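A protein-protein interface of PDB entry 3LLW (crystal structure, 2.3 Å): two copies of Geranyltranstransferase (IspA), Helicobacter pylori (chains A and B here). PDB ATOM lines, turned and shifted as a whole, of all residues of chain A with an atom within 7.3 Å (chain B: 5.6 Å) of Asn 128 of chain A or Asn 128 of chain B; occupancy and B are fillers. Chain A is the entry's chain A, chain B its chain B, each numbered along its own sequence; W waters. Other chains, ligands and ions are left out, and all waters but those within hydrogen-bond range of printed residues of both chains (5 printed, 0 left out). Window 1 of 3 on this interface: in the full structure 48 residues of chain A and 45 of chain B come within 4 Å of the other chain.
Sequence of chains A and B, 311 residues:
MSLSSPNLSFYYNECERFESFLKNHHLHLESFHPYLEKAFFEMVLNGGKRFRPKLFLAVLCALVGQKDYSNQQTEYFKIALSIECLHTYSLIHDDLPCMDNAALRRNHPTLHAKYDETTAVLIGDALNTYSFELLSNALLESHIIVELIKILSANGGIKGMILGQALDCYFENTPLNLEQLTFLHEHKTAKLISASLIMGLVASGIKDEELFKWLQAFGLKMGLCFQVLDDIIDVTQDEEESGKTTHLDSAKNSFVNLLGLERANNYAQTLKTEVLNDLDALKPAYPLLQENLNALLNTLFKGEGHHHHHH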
ATOM      1  N   PHE A  40       7.267 -22.382  -1.702  1.00  0.00           N
ATOM      2  CA  PHE A  40       8.579 -22.191  -1.061  1.00  0.00           C
ATOM      3  C   PHE A  40       8.508 -21.867   0.433  1.00  0.00           C
ATOM      4  O   PHE A  40       9.127 -22.556   1.233  1.00  0.00           O
ATOM      5  CB  PHE A  40       9.408 -21.121  -1.796  1.00  0.00           C
ATOM      6  CG  PHE A  40      10.753 -20.850  -1.169  1.00  0.00           C
ATOM      7  CD1 PHE A  40      11.709 -21.868  -1.052  1.00  0.00           C
ATOM      8  CD2 PHE A  40      11.069 -19.577  -0.698  1.00  0.00           C
ATOM      9  CE1 PHE A  40      12.949 -21.617  -0.481  1.00  0.00           C
ATOM     10  CE2 PHE A  40      12.314 -19.311  -0.120  1.00  0.00           C
ATOM     11  CZ  PHE A  40      13.256 -20.324  -0.010  1.00  0.00           C
ATOM     12  N   SER A  82      17.048 -17.615   9.363  1.00  0.00           N
ATOM     13  CA  SER A  82      17.847 -18.700   8.776  1.00  0.00           C
ATOM     14  C   SER A  82      17.747 -19.964   9.609  1.00  0.00           C
ATOM     15  O   SER A  82      17.688 -21.063   9.063  1.00  0.00           O
ATOM     16  CB  SER A  82      19.307 -18.303   8.638  1.00  0.00           C
ATOM     17  OG  SER A  82      19.932 -18.352   9.892  1.00  0.00           O
ATOM     18  N   CYS A  85      14.207 -21.461   8.957  1.00  0.00           N
ATOM     19  CA  CYS A  85      14.210 -22.175   7.664  1.00  0.00           C
ATOM     20  C   CYS A  85      14.842 -23.570   7.708  1.00  0.00           C
ATOM     21  O   CYS A  85      14.280 -24.529   7.155  1.00  0.00           O
ATOM     22  CB  CYS A  85      14.882 -21.332   6.575  1.00  0.00           C
ATOM     23  SG  CYS A  85      13.881 -19.929   6.088  1.00  0.00           S
ATOM     24  N   LEU A  86      15.996 -23.676   8.365  1.00  0.00           N
ATOM     25  CA  LEU A  86      16.648 -24.967   8.574  1.00  0.00           C
ATOM     26  C   LEU A  86      15.768 -25.923   9.360  1.00  0.00           C
ATOM     27  O   LEU A  86      15.661 -27.087   9.006  1.00  0.00           O
ATOM     28  CB  LEU A  86      17.997 -24.805   9.275  1.00  0.00           C
ATOM     29  CG  LEU A  86      18.974 -25.953   9.005  1.00  0.00           C
ATOM     30  CD1 LEU A  86      19.435 -25.932   7.556  1.00  0.00           C
ATOM     31  CD2 LEU A  86      20.171 -25.886   9.935  1.00  0.00           C
ATOM     32  N   THR A  88      12.484 -25.800   9.505  1.00  0.00           N
ATOM     33  CA  THR A  88      11.311 -26.080   8.677  1.00  0.00           C
ATOM     34  C   THR A  88      11.616 -27.114   7.600  1.00  0.00           C
ATOM     35  O   THR A  88      10.795 -27.997   7.337  1.00  0.00           O
ATOM     36  CB  THR A  88      10.793 -24.791   8.008  1.00  0.00           C
ATOM     37  OG1 THR A  88      10.714 -23.756   8.989  1.00  0.00           O
ATOM     38  CG2 THR A  88       9.417 -25.009   7.388  1.00  0.00           C
ATOM     39  N   TYR A  89      12.793 -27.002   6.980  1.00  0.00           N
ATOM     40  CA  TYR A  89      13.201 -27.932   5.919  1.00  0.00           C
ATOM     41  C   TYR A  89      13.290 -29.353   6.465  1.00  0.00           C
ATOM     42  O   TYR A  89      12.868 -30.309   5.787  1.00  0.00           O
ATOM     43  CB  TYR A  89      14.516 -27.507   5.231  1.00  0.00           C
ATOM     44  CG  TYR A  89      15.692 -28.460   5.431  1.00  0.00           C
ATOM     45  CD1 TYR A  89      15.742 -29.700   4.782  1.00  0.00           C
ATOM     46  CD2 TYR A  89      16.762 -28.111   6.250  1.00  0.00           C
ATOM     47  CE1 TYR A  89      16.778 -30.572   4.971  1.00  0.00           C
ATOM     48  CE2 TYR A  89      17.811 -28.984   6.454  1.00  0.00           C
ATOM     49  CZ  TYR A  89      17.832 -30.192   5.793  1.00  0.00           C
ATOM     50  OH  TYR A  89      18.858 -31.058   5.976  1.00  0.00           O
ATOM     51  N   SER A  90      13.841 -29.497   7.673  1.00  0.00           N
ATOM     52  CA  SER A  90      13.894 -30.810   8.308  1.00  0.00           C
ATOM     53  C   SER A  90      12.489 -31.408   8.493  1.00  0.00           C
ATOM     54  O   SER A  90      12.293 -32.608   8.282  1.00  0.00           O
ATOM     55  CB  SER A  90      14.655 -30.767   9.625  1.00  0.00           C
ATOM     56  OG  SER A  90      13.945 -30.006  10.568  1.00  0.00           O
ATOM     57  N   HIS A  93      11.046 -32.695   5.142  1.00  0.00           N
ATOM     58  CA  HIS A  93      11.602 -33.997   4.799  1.00  0.00           C
ATOM     59  C   HIS A  93      11.155 -35.101   5.746  1.00  0.00           C
ATOM     60  O   HIS A  93      10.868 -36.211   5.298  1.00  0.00           O
ATOM     61  CB  HIS A  93      13.121 -33.914   4.609  1.00  0.00           C
ATOM     62  CG  HIS A  93      13.503 -33.245   3.325  1.00  0.00           C
ATOM     63  ND1 HIS A  93      14.767 -33.310   2.791  1.00  0.00           N
ATOM     64  CD2 HIS A  93      12.756 -32.543   2.436  1.00  0.00           C
ATOM     65  CE1 HIS A  93      14.796 -32.648   1.648  1.00  0.00           C
ATOM     66  NE2 HIS A  93      13.588 -32.177   1.408  1.00  0.00           N
ATOM     67  N   LEU A 122      12.317 -30.995  -3.057  1.00  0.00           N
ATOM     68  CA  LEU A 122      13.018 -29.851  -3.628  1.00  0.00           C
ATOM     69  C   LEU A 122      12.846 -28.565  -2.831  1.00  0.00           C
ATOM     70  O   LEU A 122      13.797 -27.788  -2.689  1.00  0.00           O
ATOM     71  CB  LEU A 122      12.636 -29.648  -5.099  1.00  0.00           C
ATOM     72  CG  LEU A 122      13.138 -30.735  -6.046  1.00  0.00           C
ATOM     73  CD1 LEU A 122      12.589 -30.499  -7.440  1.00  0.00           C
ATOM     74  CD2 LEU A 122      14.695 -30.866  -6.046  1.00  0.00           C
ATOM     75  N   ILE A 123      11.650 -28.346  -2.300  1.00  0.00           N
ATOM     76  CA  ILE A 123      11.439 -27.219  -1.379  1.00  0.00           C
ATOM     77  C   ILE A 123      12.157 -27.344  -0.030  1.00  0.00           C
ATOM     78  O   ILE A 123      12.719 -26.350   0.450  1.00  0.00           O
ATOM     79  CB  ILE A 123       9.969 -26.786  -1.292  1.00  0.00           C
ATOM     80  CG1 ILE A 123       9.692 -25.871  -2.480  1.00  0.00           C
ATOM     81  CG2 ILE A 123       9.678 -25.992  -0.028  1.00  0.00           C
ATOM     82  CD1 ILE A 123       8.296 -25.912  -2.918  1.00  0.00           C
ATOM     83  N   GLY A 124      12.196 -28.546   0.553  1.00  0.00           N
ATOM     84  CA  GLY A 124      13.090 -28.774   1.705  1.00  0.00           C
ATOM     85  C   GLY A 124      14.555 -28.488   1.360  1.00  0.00           C
ATOM     86  O   GLY A 124      15.282 -27.863   2.134  1.00  0.00           O
ATOM     87  N   ASP A 125      14.985 -28.937   0.184  1.00  0.00           N
ATOM     88  CA  ASP A 125      16.332 -28.686  -0.329  1.00  0.00           C
ATOM     89  C   ASP A 125      16.649 -27.203  -0.461  1.00  0.00           C
ATOM     90  O   ASP A 125      17.724 -26.755  -0.050  1.00  0.00           O
ATOM     91  CB  ASP A 125      16.530 -29.363  -1.683  1.00  0.00           C
ATOM     92  CG  ASP A 125      16.741 -30.854  -1.570  1.00  0.00           C
ATOM     93  OD1 ASP A 125      16.827 -31.361  -0.431  1.00  0.00           O
ATOM     94  OD2 ASP A 125      16.826 -31.519  -2.631  1.00  0.00           O
ATOM     95  N   ALA A 126      15.708 -26.456  -1.034  1.00  0.00           N
ATOM     96  CA  ALA A 126      15.832 -25.006  -1.166  1.00  0.00           C
ATOM     97  C   ALA A 126      15.856 -24.276   0.159  1.00  0.00           C
ATOM     98  O   ALA A 126      16.653 -23.313   0.341  1.00  0.00           O
ATOM     99  CB  ALA A 126      14.758 -24.451  -2.051  1.00  0.00           C
ATOM    100  N   LEU A 127      15.000 -24.710   1.087  1.00  0.00           N
ATOM    101  CA  LEU A 127      15.016 -24.086   2.418  1.00  0.00           C
ATOM    102  C   LEU A 127      16.306 -24.328   3.219  1.00  0.00           C
ATOM    103  O   LEU A 127      16.742 -23.461   3.984  1.00  0.00           O
ATOM    104  CB  LEU A 127      13.783 -24.461   3.222  1.00  0.00           C
ATOM    105  CG  LEU A 127      12.511 -23.684   2.858  1.00  0.00           C
ATOM    106  CD1 LEU A 127      11.325 -24.340   3.514  1.00  0.00           C
ATOM    107  CD2 LEU A 127      12.610 -22.203   3.262  1.00  0.00           C
ATOM    108  N   ASN A 128      16.890 -25.509   3.040  1.00  0.00           N
ATOM    109  CA  ASN A 128      18.219 -25.842   3.534  1.00  0.00           C
ATOM    110  C   ASN A 128      19.270 -24.874   2.988  1.00  0.00           C
ATOM    111  O   ASN A 128      19.986 -24.287   3.769  1.00  0.00           O
ATOM    112  CB  ASN A 128      18.561 -27.267   3.116  1.00  0.00           C
ATOM    113  CG  ASN A 128      19.880 -27.777   3.670  1.00  0.00           C
ATOM    114  OD1 ASN A 128      20.632 -27.083   4.386  1.00  0.00           O
ATOM    115  ND2 ASN A 128      20.176 -29.015   3.323  1.00  0.00           N
ATOM    116  N   THR A 129      19.357 -24.732   1.659  1.00  0.00           N
ATOM    117  CA  THR A 129      20.284 -23.788   1.009  1.00  0.00           C
ATOM    118  C   THR A 129      19.972 -22.330   1.333  1.00  0.00           C
ATOM    119  O   THR A 129      20.899 -21.492   1.559  1.00  0.00           O
ATOM    120  CB  THR A 129      20.311 -23.992  -0.530  1.00  0.00           C
ATOM    121  OG1 THR A 129      20.486 -25.380  -0.813  1.00  0.00           O
ATOM    122  CG2 THR A 129      21.458 -23.238  -1.160  1.00  0.00           C
ATOM    123  N   TYR A 130      18.678 -22.025   1.393  1.00  0.00           N
ATOM    124  CA  TYR A 130      18.211 -20.645   1.718  1.00  0.00           C
ATOM    125  C   TYR A 130      18.677 -20.076   3.059  1.00  0.00           C
ATOM    126  O   TYR A 130      18.900 -18.873   3.154  1.00  0.00           O
ATOM    127  CB  TYR A 130      16.693 -20.503   1.601  1.00  0.00           C
ATOM    128  CG  TYR A 130      16.214 -19.074   1.509  1.00  0.00           C
ATOM    129  CD1 TYR A 130      15.332 -18.561   2.444  1.00  0.00           C
ATOM    130  CD2 TYR A 130      16.656 -18.234   0.489  1.00  0.00           C
ATOM    131  CE1 TYR A 130      14.883 -17.244   2.359  1.00  0.00           C
ATOM    132  CE2 TYR A 130      16.231 -16.914   0.403  1.00  0.00           C
ATOM    133  CZ  TYR A 130      15.344 -16.427   1.346  1.00  0.00           C
ATOM    134  OH  TYR A 130      14.914 -15.116   1.267  1.00  0.00           O
ATOM    135  N   SER A 131      18.795 -20.931   4.080  1.00  0.00           N
ATOM    136  CA  SER A 131      19.315 -20.556   5.407  1.00  0.00           C
ATOM    137  C   SER A 131      20.704 -19.950   5.324  1.00  0.00           C
ATOM    138  O   SER A 131      21.059 -19.066   6.081  1.00  0.00           O
ATOM    139  CB  SER A 131      19.422 -21.796   6.291  1.00  0.00           C
ATOM    140  OG  SER A 131      18.229 -22.547   6.249  1.00  0.00           O
ATOM    141  N   PHE A 132      21.491 -20.452   4.385  1.00  0.00           N
ATOM    142  CA  PHE A 132      22.844 -19.989   4.200  1.00  0.00           C
ATOM    143  C   PHE A 132      22.913 -18.730   3.357  1.00  0.00           C
ATOM    144  O   PHE A 132      23.784 -17.865   3.593  1.00  0.00           O
ATOM    145  CB  PHE A 132      23.728 -21.156   3.728  1.00  0.00           C
ATOM    146  CG  PHE A 132      23.690 -22.333   4.690  1.00  0.00           C
ATOM    147  CD1 PHE A 132      24.396 -22.285   5.882  1.00  0.00           C
ATOM    148  CD2 PHE A 132      22.866 -23.451   4.442  1.00  0.00           C
ATOM    149  CE1 PHE A 132      24.341 -23.337   6.804  1.00  0.00           C
ATOM    150  CE2 PHE A 132      22.803 -24.517   5.363  1.00  0.00           C
ATOM    151  CZ  PHE A 132      23.553 -24.465   6.540  1.00  0.00           C
ATOM    152  N   GLU A 133      21.960 -18.582   2.437  1.00  0.00           N
ATOM    153  CA  GLU A 133      21.803 -17.348   1.669  1.00  0.00           C
ATOM    154  C   GLU A 133      21.355 -16.208   2.562  1.00  0.00           C
ATOM    155  O   GLU A 133      21.924 -15.118   2.488  1.00  0.00           O
ATOM    156  CB  GLU A 133      20.831 -17.509   0.497  1.00  0.00           C
ATOM    157  CG  GLU A 133      20.830 -16.302  -0.469  1.00  0.00           C
ATOM    158  CD  GLU A 133      19.974 -16.503  -1.722  1.00  0.00           C
ATOM    159  OE1 GLU A 133      19.115 -17.419  -1.753  1.00  0.00           O
ATOM    160  OE2 GLU A 133      20.168 -15.726  -2.683  1.00  0.00           O
ATOM    161  N   LEU A 152      25.943 -23.027  12.270  1.00  0.00           N
ATOM    162  CA  LEU A 152      24.677 -23.584  11.752  1.00  0.00           C
ATOM    163  C   LEU A 152      24.883 -24.818  10.863  1.00  0.00           C
ATOM    164  O   LEU A 152      24.184 -25.830  11.014  1.00  0.00           O
ATOM    165  CB  LEU A 152      23.870 -22.506  11.021  1.00  0.00           C
ATOM    166  CG  LEU A 152      22.421 -22.909  10.685  1.00  0.00           C
ATOM    167  CD1 LEU A 152      21.513 -22.946  11.927  1.00  0.00           C
ATOM    168  CD2 LEU A 152      21.845 -21.987   9.633  1.00  0.00           C
ATOM    169  N   GLY A 156      23.539 -28.374  12.041  1.00  0.00           N
ATOM    170  CA  GLY A 156      22.352 -28.728  11.267  1.00  0.00           C
ATOM    171  C   GLY A 156      22.668 -29.826  10.281  1.00  0.00           C
ATOM    172  O   GLY A 156      21.777 -30.356   9.628  1.00  0.00           O
ATOM    173  N   MET A 161      22.042 -32.509  13.332  1.00  0.00           N
ATOM    174  CA  MET A 161      20.598 -32.718  13.164  1.00  0.00           C
ATOM    175  C   MET A 161      20.248 -33.864  12.226  1.00  0.00           C
ATOM    176  O   MET A 161      19.378 -34.678  12.538  1.00  0.00           O
ATOM    177  CB  MET A 161      19.941 -31.409  12.732  1.00  0.00           C
ATOM    178  CG  MET A 161      18.437 -31.450  12.579  1.00  0.00           C
ATOM    179  SD  MET A 161      17.798 -29.937  11.819  1.00  0.00           S
ATOM    180  CE  MET A 161      18.386 -30.204  10.134  1.00  0.00           C
ATOM    181  N   ILE A 162      20.978 -33.962  11.114  1.00  0.00           N
ATOM    182  CA  ILE A 162      20.774 -35.016  10.117  1.00  0.00           C
ATOM    183  C   ILE A 162      21.103 -36.417  10.646  1.00  0.00           C
ATOM    184  O   ILE A 162      20.287 -37.347  10.479  1.00  0.00           O
ATOM    185  CB  ILE A 162      21.484 -34.693   8.790  1.00  0.00           C
ATOM    186  CG1 ILE A 162      20.737 -33.568   8.087  1.00  0.00           C
ATOM    187  CG2 ILE A 162      21.513 -35.896   7.856  1.00  0.00           C
ATOM    188  CD1 ILE A 162      21.605 -32.772   7.141  1.00  0.00           C
ATOM    189  N   CYS B  85      30.396 -31.169  -3.843  1.00  0.00           N
ATOM    190  CA  CYS B  85      29.388 -31.697  -2.902  1.00  0.00           C
ATOM    191  C   CYS B  85      27.973 -31.237  -3.248  1.00  0.00           C
ATOM    192  O   CYS B  85      27.048 -32.050  -3.249  1.00  0.00           O
ATOM    193  CB  CYS B  85      29.718 -31.329  -1.463  1.00  0.00           C
ATOM    194  SG  CYS B  85      31.170 -32.200  -0.823  1.00  0.00           S
ATOM    195  N   LEU B  86      27.817 -29.953  -3.561  1.00  0.00           N
ATOM    196  CA  LEU B  86      26.512 -29.394  -3.942  1.00  0.00           C
ATOM    197  C   LEU B  86      26.016 -30.022  -5.232  1.00  0.00           C
ATOM    198  O   LEU B  86      24.851 -30.461  -5.327  1.00  0.00           O
ATOM    199  CB  LEU B  86      26.584 -27.870  -4.087  1.00  0.00           C
ATOM    200  CG  LEU B  86      25.238 -27.166  -3.981  1.00  0.00           C
ATOM    201  CD1 LEU B  86      24.716 -27.200  -2.561  1.00  0.00           C
ATOM    202  CD2 LEU B  86      25.348 -25.752  -4.457  1.00  0.00           C
ATOM    203  N   TYR B  89      25.060 -33.685  -4.354  1.00  0.00           N
ATOM    204  CA  TYR B  89      23.765 -33.751  -3.650  1.00  0.00           C
ATOM    205  C   TYR B  89      22.622 -33.725  -4.654  1.00  0.00           C
ATOM    206  O   TYR B  89      21.644 -34.475  -4.499  1.00  0.00           O
ATOM    207  CB  TYR B  89      23.580 -32.679  -2.539  1.00  0.00           C
ATOM    208  CG  TYR B  89      22.445 -31.651  -2.734  1.00  0.00           C
ATOM    209  CD1 TYR B  89      21.102 -32.030  -2.684  1.00  0.00           C
ATOM    210  CD2 TYR B  89      22.737 -30.291  -2.958  1.00  0.00           C
ATOM    211  CE1 TYR B  89      20.075 -31.112  -2.895  1.00  0.00           C
ATOM    212  CE2 TYR B  89      21.725 -29.358  -3.145  1.00  0.00           C
ATOM    213  CZ  TYR B  89      20.384 -29.795  -3.129  1.00  0.00           C
ATOM    214  OH  TYR B  89      19.353 -28.918  -3.312  1.00  0.00           O
ATOM    215  N   ILE B 123      21.249 -38.044   3.037  1.00  0.00           N
ATOM    216  CA  ILE B 123      22.643 -37.827   2.624  1.00  0.00           C
ATOM    217  C   ILE B 123      22.766 -36.732   1.585  1.00  0.00           C
ATOM    218  O   ILE B 123      23.704 -35.912   1.643  1.00  0.00           O
ATOM    219  CB  ILE B 123      23.362 -39.129   2.254  1.00  0.00           C
ATOM    220  CG1 ILE B 123      23.704 -39.834   3.565  1.00  0.00           C
ATOM    221  CG2 ILE B 123      24.653 -38.872   1.408  1.00  0.00           C
ATOM    222  CD1 ILE B 123      24.102 -41.211   3.386  1.00  0.00           C
ATOM    223  N   GLY B 124      21.794 -36.691   0.675  1.00  0.00           N
ATOM    224  CA  GLY B 124      21.583 -35.517  -0.191  1.00  0.00           C
ATOM    225  C   GLY B 124      21.483 -34.230   0.622  1.00  0.00           C
ATOM    226  O   GLY B 124      22.150 -33.238   0.288  1.00  0.00           O
ATOM    227  N   ASP B 125      20.667 -34.236   1.689  1.00  0.00           N
ATOM    228  CA  ASP B 125      20.505 -33.053   2.567  1.00  0.00           C
ATOM    229  C   ASP B 125      21.854 -32.704   3.257  1.00  0.00           C
ATOM    230  O   ASP B 125      22.186 -31.530   3.423  1.00  0.00           O
ATOM    231  CB  ASP B 125      19.446 -33.306   3.661  1.00  0.00           C
ATOM    232  CG  ASP B 125      18.019 -33.576   3.099  1.00  0.00           C
ATOM    233  OD1 ASP B 125      17.731 -33.202   1.945  1.00  0.00           O
ATOM    234  OD2 ASP B 125      17.170 -34.149   3.831  1.00  0.00           O
ATOM    235  N   ALA B 126      22.592 -33.727   3.676  1.00  0.00           N
ATOM    236  CA  ALA B 126      23.870 -33.544   4.416  1.00  0.00           C
ATOM    237  C   ALA B 126      24.936 -32.961   3.543  1.00  0.00           C
ATOM    238  O   ALA B 126      25.606 -32.037   3.949  1.00  0.00           O
ATOM    239  CB  ALA B 126      24.353 -34.856   5.022  1.00  0.00           C
ATOM    240  N   LEU B 127      25.056 -33.482   2.325  1.00  0.00           N
ATOM    241  CA  LEU B 127      25.954 -32.914   1.313  1.00  0.00           C
ATOM    242  C   LEU B 127      25.598 -31.488   0.880  1.00  0.00           C
ATOM    243  O   LEU B 127      26.529 -30.651   0.671  1.00  0.00           O
ATOM    244  CB  LEU B 127      26.089 -33.840   0.098  1.00  0.00           C
ATOM    245  CG  LEU B 127      26.965 -35.083   0.307  1.00  0.00           C
ATOM    246  CD1 LEU B 127      26.824 -36.028  -0.863  1.00  0.00           C
ATOM    247  CD2 LEU B 127      28.441 -34.728   0.532  1.00  0.00           C
ATOM    248  N   ASN B 128      24.290 -31.197   0.736  1.00  0.00           N
ATOM    249  CA  ASN B 128      23.864 -29.778   0.592  1.00  0.00           C
ATOM    250  C   ASN B 128      24.484 -28.886   1.707  1.00  0.00           C
ATOM    251  O   ASN B 128      25.163 -27.926   1.415  1.00  0.00           O
ATOM    252  CB  ASN B 128      22.340 -29.640   0.590  1.00  0.00           C
ATOM    253  CG  ASN B 128      21.849 -28.232   0.206  1.00  0.00           C
ATOM    254  OD1 ASN B 128      22.629 -27.314  -0.045  1.00  0.00           O
ATOM    255  ND2 ASN B 128      20.537 -28.063   0.186  1.00  0.00           N
ATOM    256  N   THR B 129      24.246 -29.235   2.973  1.00  0.00           N
ATOM    257  CA  THR B 129      24.673 -28.448   4.125  1.00  0.00           C
ATOM    258  C   THR B 129      26.202 -28.438   4.293  1.00  0.00           C
ATOM    259  O   THR B 129      26.782 -27.411   4.643  1.00  0.00           O
ATOM    260  CB  THR B 129      23.983 -28.994   5.405  1.00  0.00           C
ATOM    261  OG1 THR B 129      22.567 -28.840   5.270  1.00  0.00           O
ATOM    262  CG2 THR B 129      24.468 -28.272   6.653  1.00  0.00           C
ATOM    263  N   TYR B 130      26.829 -29.583   4.014  1.00  0.00           N
ATOM    264  CA  TYR B 130      28.288 -29.756   4.023  1.00  0.00           C
ATOM    265  C   TYR B 130      29.042 -28.861   3.038  1.00  0.00           C
ATOM    266  O   TYR B 130      30.154 -28.384   3.355  1.00  0.00           O
ATOM    267  CB  TYR B 130      28.669 -31.235   3.836  1.00  0.00           C
ATOM    268  CG  TYR B 130      30.099 -31.563   4.228  1.00  0.00           C
ATOM    269  CD1 TYR B 130      31.034 -32.006   3.276  1.00  0.00           C
ATOM    270  CD2 TYR B 130      30.522 -31.419   5.545  1.00  0.00           C
ATOM    271  CE1 TYR B 130      32.367 -32.302   3.647  1.00  0.00           C
ATOM    272  CE2 TYR B 130      31.840 -31.692   5.914  1.00  0.00           C
ATOM    273  CZ  TYR B 130      32.756 -32.131   4.966  1.00  0.00           C
ATOM    274  OH  TYR B 130      34.048 -32.409   5.370  1.00  0.00           O
ATOM    275  N   SER B 131      28.461 -28.607   1.858  1.00  0.00           N
ATOM    276  CA  SER B 131      29.016 -27.553   0.975  1.00  0.00           C
ATOM    277  C   SER B 131      29.333 -26.267   1.761  1.00  0.00           C
ATOM    278  O   SER B 131      30.436 -25.711   1.684  1.00  0.00           O
ATOM    279  CB  SER B 131      28.053 -27.213  -0.147  1.00  0.00           C
ATOM    280  OG  SER B 131      27.698 -28.365  -0.868  1.00  0.00           O
ATOM    281  N   PHE B 132      28.367 -25.821   2.551  1.00  0.00           N
ATOM    282  CA  PHE B 132      28.502 -24.573   3.307  1.00  0.00           C
ATOM    283  C   PHE B 132      29.421 -24.654   4.494  1.00  0.00           C
ATOM    284  O   PHE B 132      30.096 -23.671   4.808  1.00  0.00           O
ATOM    285  CB  PHE B 132      27.131 -23.982   3.610  1.00  0.00           C
ATOM    286  CG  PHE B 132      26.330 -23.773   2.353  1.00  0.00           C
ATOM    287  CD1 PHE B 132      26.645 -22.718   1.493  1.00  0.00           C
ATOM    288  CD2 PHE B 132      25.344 -24.691   1.970  1.00  0.00           C
ATOM    289  CE1 PHE B 132      25.960 -22.547   0.306  1.00  0.00           C
ATOM    290  CE2 PHE B 132      24.655 -24.527   0.774  1.00  0.00           C
ATOM    291  CZ  PHE B 132      24.967 -23.455  -0.061  1.00  0.00           C
HETATM  292  O   HOH W   1      17.909 -30.849  -5.214  1.00  0.00           O
HETATM  293  O   HOH W   2      16.699 -33.409   6.479  1.00  0.00           O
HETATM  294  O   HOH W   3      18.825 -30.474   1.036  1.00  0.00           O
HETATM  295  O   HOH W   4      20.776 -29.654   7.126  1.00  0.00           O
HETATM  296  O   HOH W   5      20.293 -26.542  -3.194  1.00  0.00           O
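ND2 of Asn 128 of chain A sits at hydrogen-bond distance from O of Asp 125 of chain B (3.2 Å). The side-chain amide nitrogen (ND2) of Asn 128 of chain B is in hydrogen-bond range of the side-chain hydroxyl (OG1) of Thr 129 of chain A. ND1 of His 93 of chain A is in hydrogen-bond range of OD2 of Asp 125 of chain B, 2.7 Å away. OD1 of Asp 125 of chain B lies close to OD1 of Asp 125 of chain A (3.1 Å). O of Asp 125 of chain A is in hydrogen-bond range of ND2 of Asn 128 of chain B, at 3.1 Å. ND2 of Asn 128 of chain B lies close to ND2 of Asn 128 of chain A, at 3.3 Å. OG1 of Thr 129 of chain B lies within hydrogen-bond range of OD1 of Asn 128 of chain A.
O of Asn 128 of chain B lies close to OG of Ser 131 of chain B (3.4 Å). The backbone carbonyl oxygen (O) of Asp 125 of chain A lies within hydrogen-bond range of the side-chain hydroxyl (OG1) of Thr 129 of chain A, 3.2 Å away. The side-chain hydroxyl (OG1) of Thr 129 of chain B sits at hydrogen-bond distance from the backbone carbonyl oxygen (O) of Asp 125 of chain B (3.3 Å).
OH of Tyr 89 of chain A touches CB of Asp 125 of chain B (3.3 Å). OD2 of Asp 125 of chain A touches CE1 of Tyr 89 of chain B (3.3 Å). CZ of Phe 132 of chain A touches CG2 of Thr 129 of chain B, 3.9 Å away. Phe 132 of chain A touches Phe 132 of chain B (CD2 to CD2, 3.7 Å). CD1 of Ile 162 of chain A touches C of Asp 125 of chain B (3.9 Å). Ile 162 of chain A touches Ala 126 of chain B (CD1 to CA, 3.6 Å).
Thr 88 of chain A touches none of the printed residues of chain B. Asn 128 of chain A touches just these residues of chain B: Asp 125 (3.2 Å), Asn 128 (3.3 Å) and Thr 129 (2.8 Å). Printed residues of chain A within 4 Å of Asp 125 of chain B: Tyr 89, His 93, Asp 125, Asn 128 and Ile 162. Of the printed residues of chain A, Ala 126 of chain B touches Ile 162. Leu 127 of chain B touches none of the printed residues of chain A. Of chain A, only Asp 125 (3.1 Å), Asn 128 (3.3 Å) and Thr 129 (2.9 Å) come within 4 Å of Asn 128 of chain B. The nearest residue of chain B that does not touch Asn 128 of chain A is Ala 126 of chain B (5.3 Å).
Printed residues of chain B that touch a printed residue of chain A: Tyr 89, Asp 125, Ala 126, Asn 128, Thr 129 and Phe 132. Of the 24 printed residues of chain A, 7 touch a printed residue of chain B. Printed residues of chain A that touch a printed residue of chain B: Tyr 89, His 93, Asp 125, Asn 128, Thr 129, Phe 132 and Ile 162. Hydrophobic or aromatic side chains of chain A within 4 Å of the printed part of chain B: Tyr 89, His 93, Phe 132 and Ile 162. Along chain A the printed residues that touch a printed residue of chain B span positions 89 to 162.
Tyr 89 of chain A touches Asp 125 of chain B, and with the chains exchanged Asp 125 of chain A touches Tyr 89 of chain B. Asn 128 of chain B touches its own counterpart, Asn 128 of chain A. Positions printed for both chains: 85, 86, 89, 123, 124, 125, 126, 127, 128, 129, 130, 131 and 132.
Water W4 lies within hydrogen-bond range of the side-chain hydroxyl of Tyr 89 of chain A, the side-chain hydroxyl of Thr 129 of chain B and the backbone carbonyl oxygen of Gly 156 of chain A. Water W2 lies within hydrogen-bond range of OD2 of Asp 125 of chain B (2.8 Å) and OH of Tyr 89 of chain A (3.2 Å). Water W1 bridges OD2 of Asp 125 of chain A (2.9 Å) and OH of Tyr 89 of chain B (3.1 Å).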
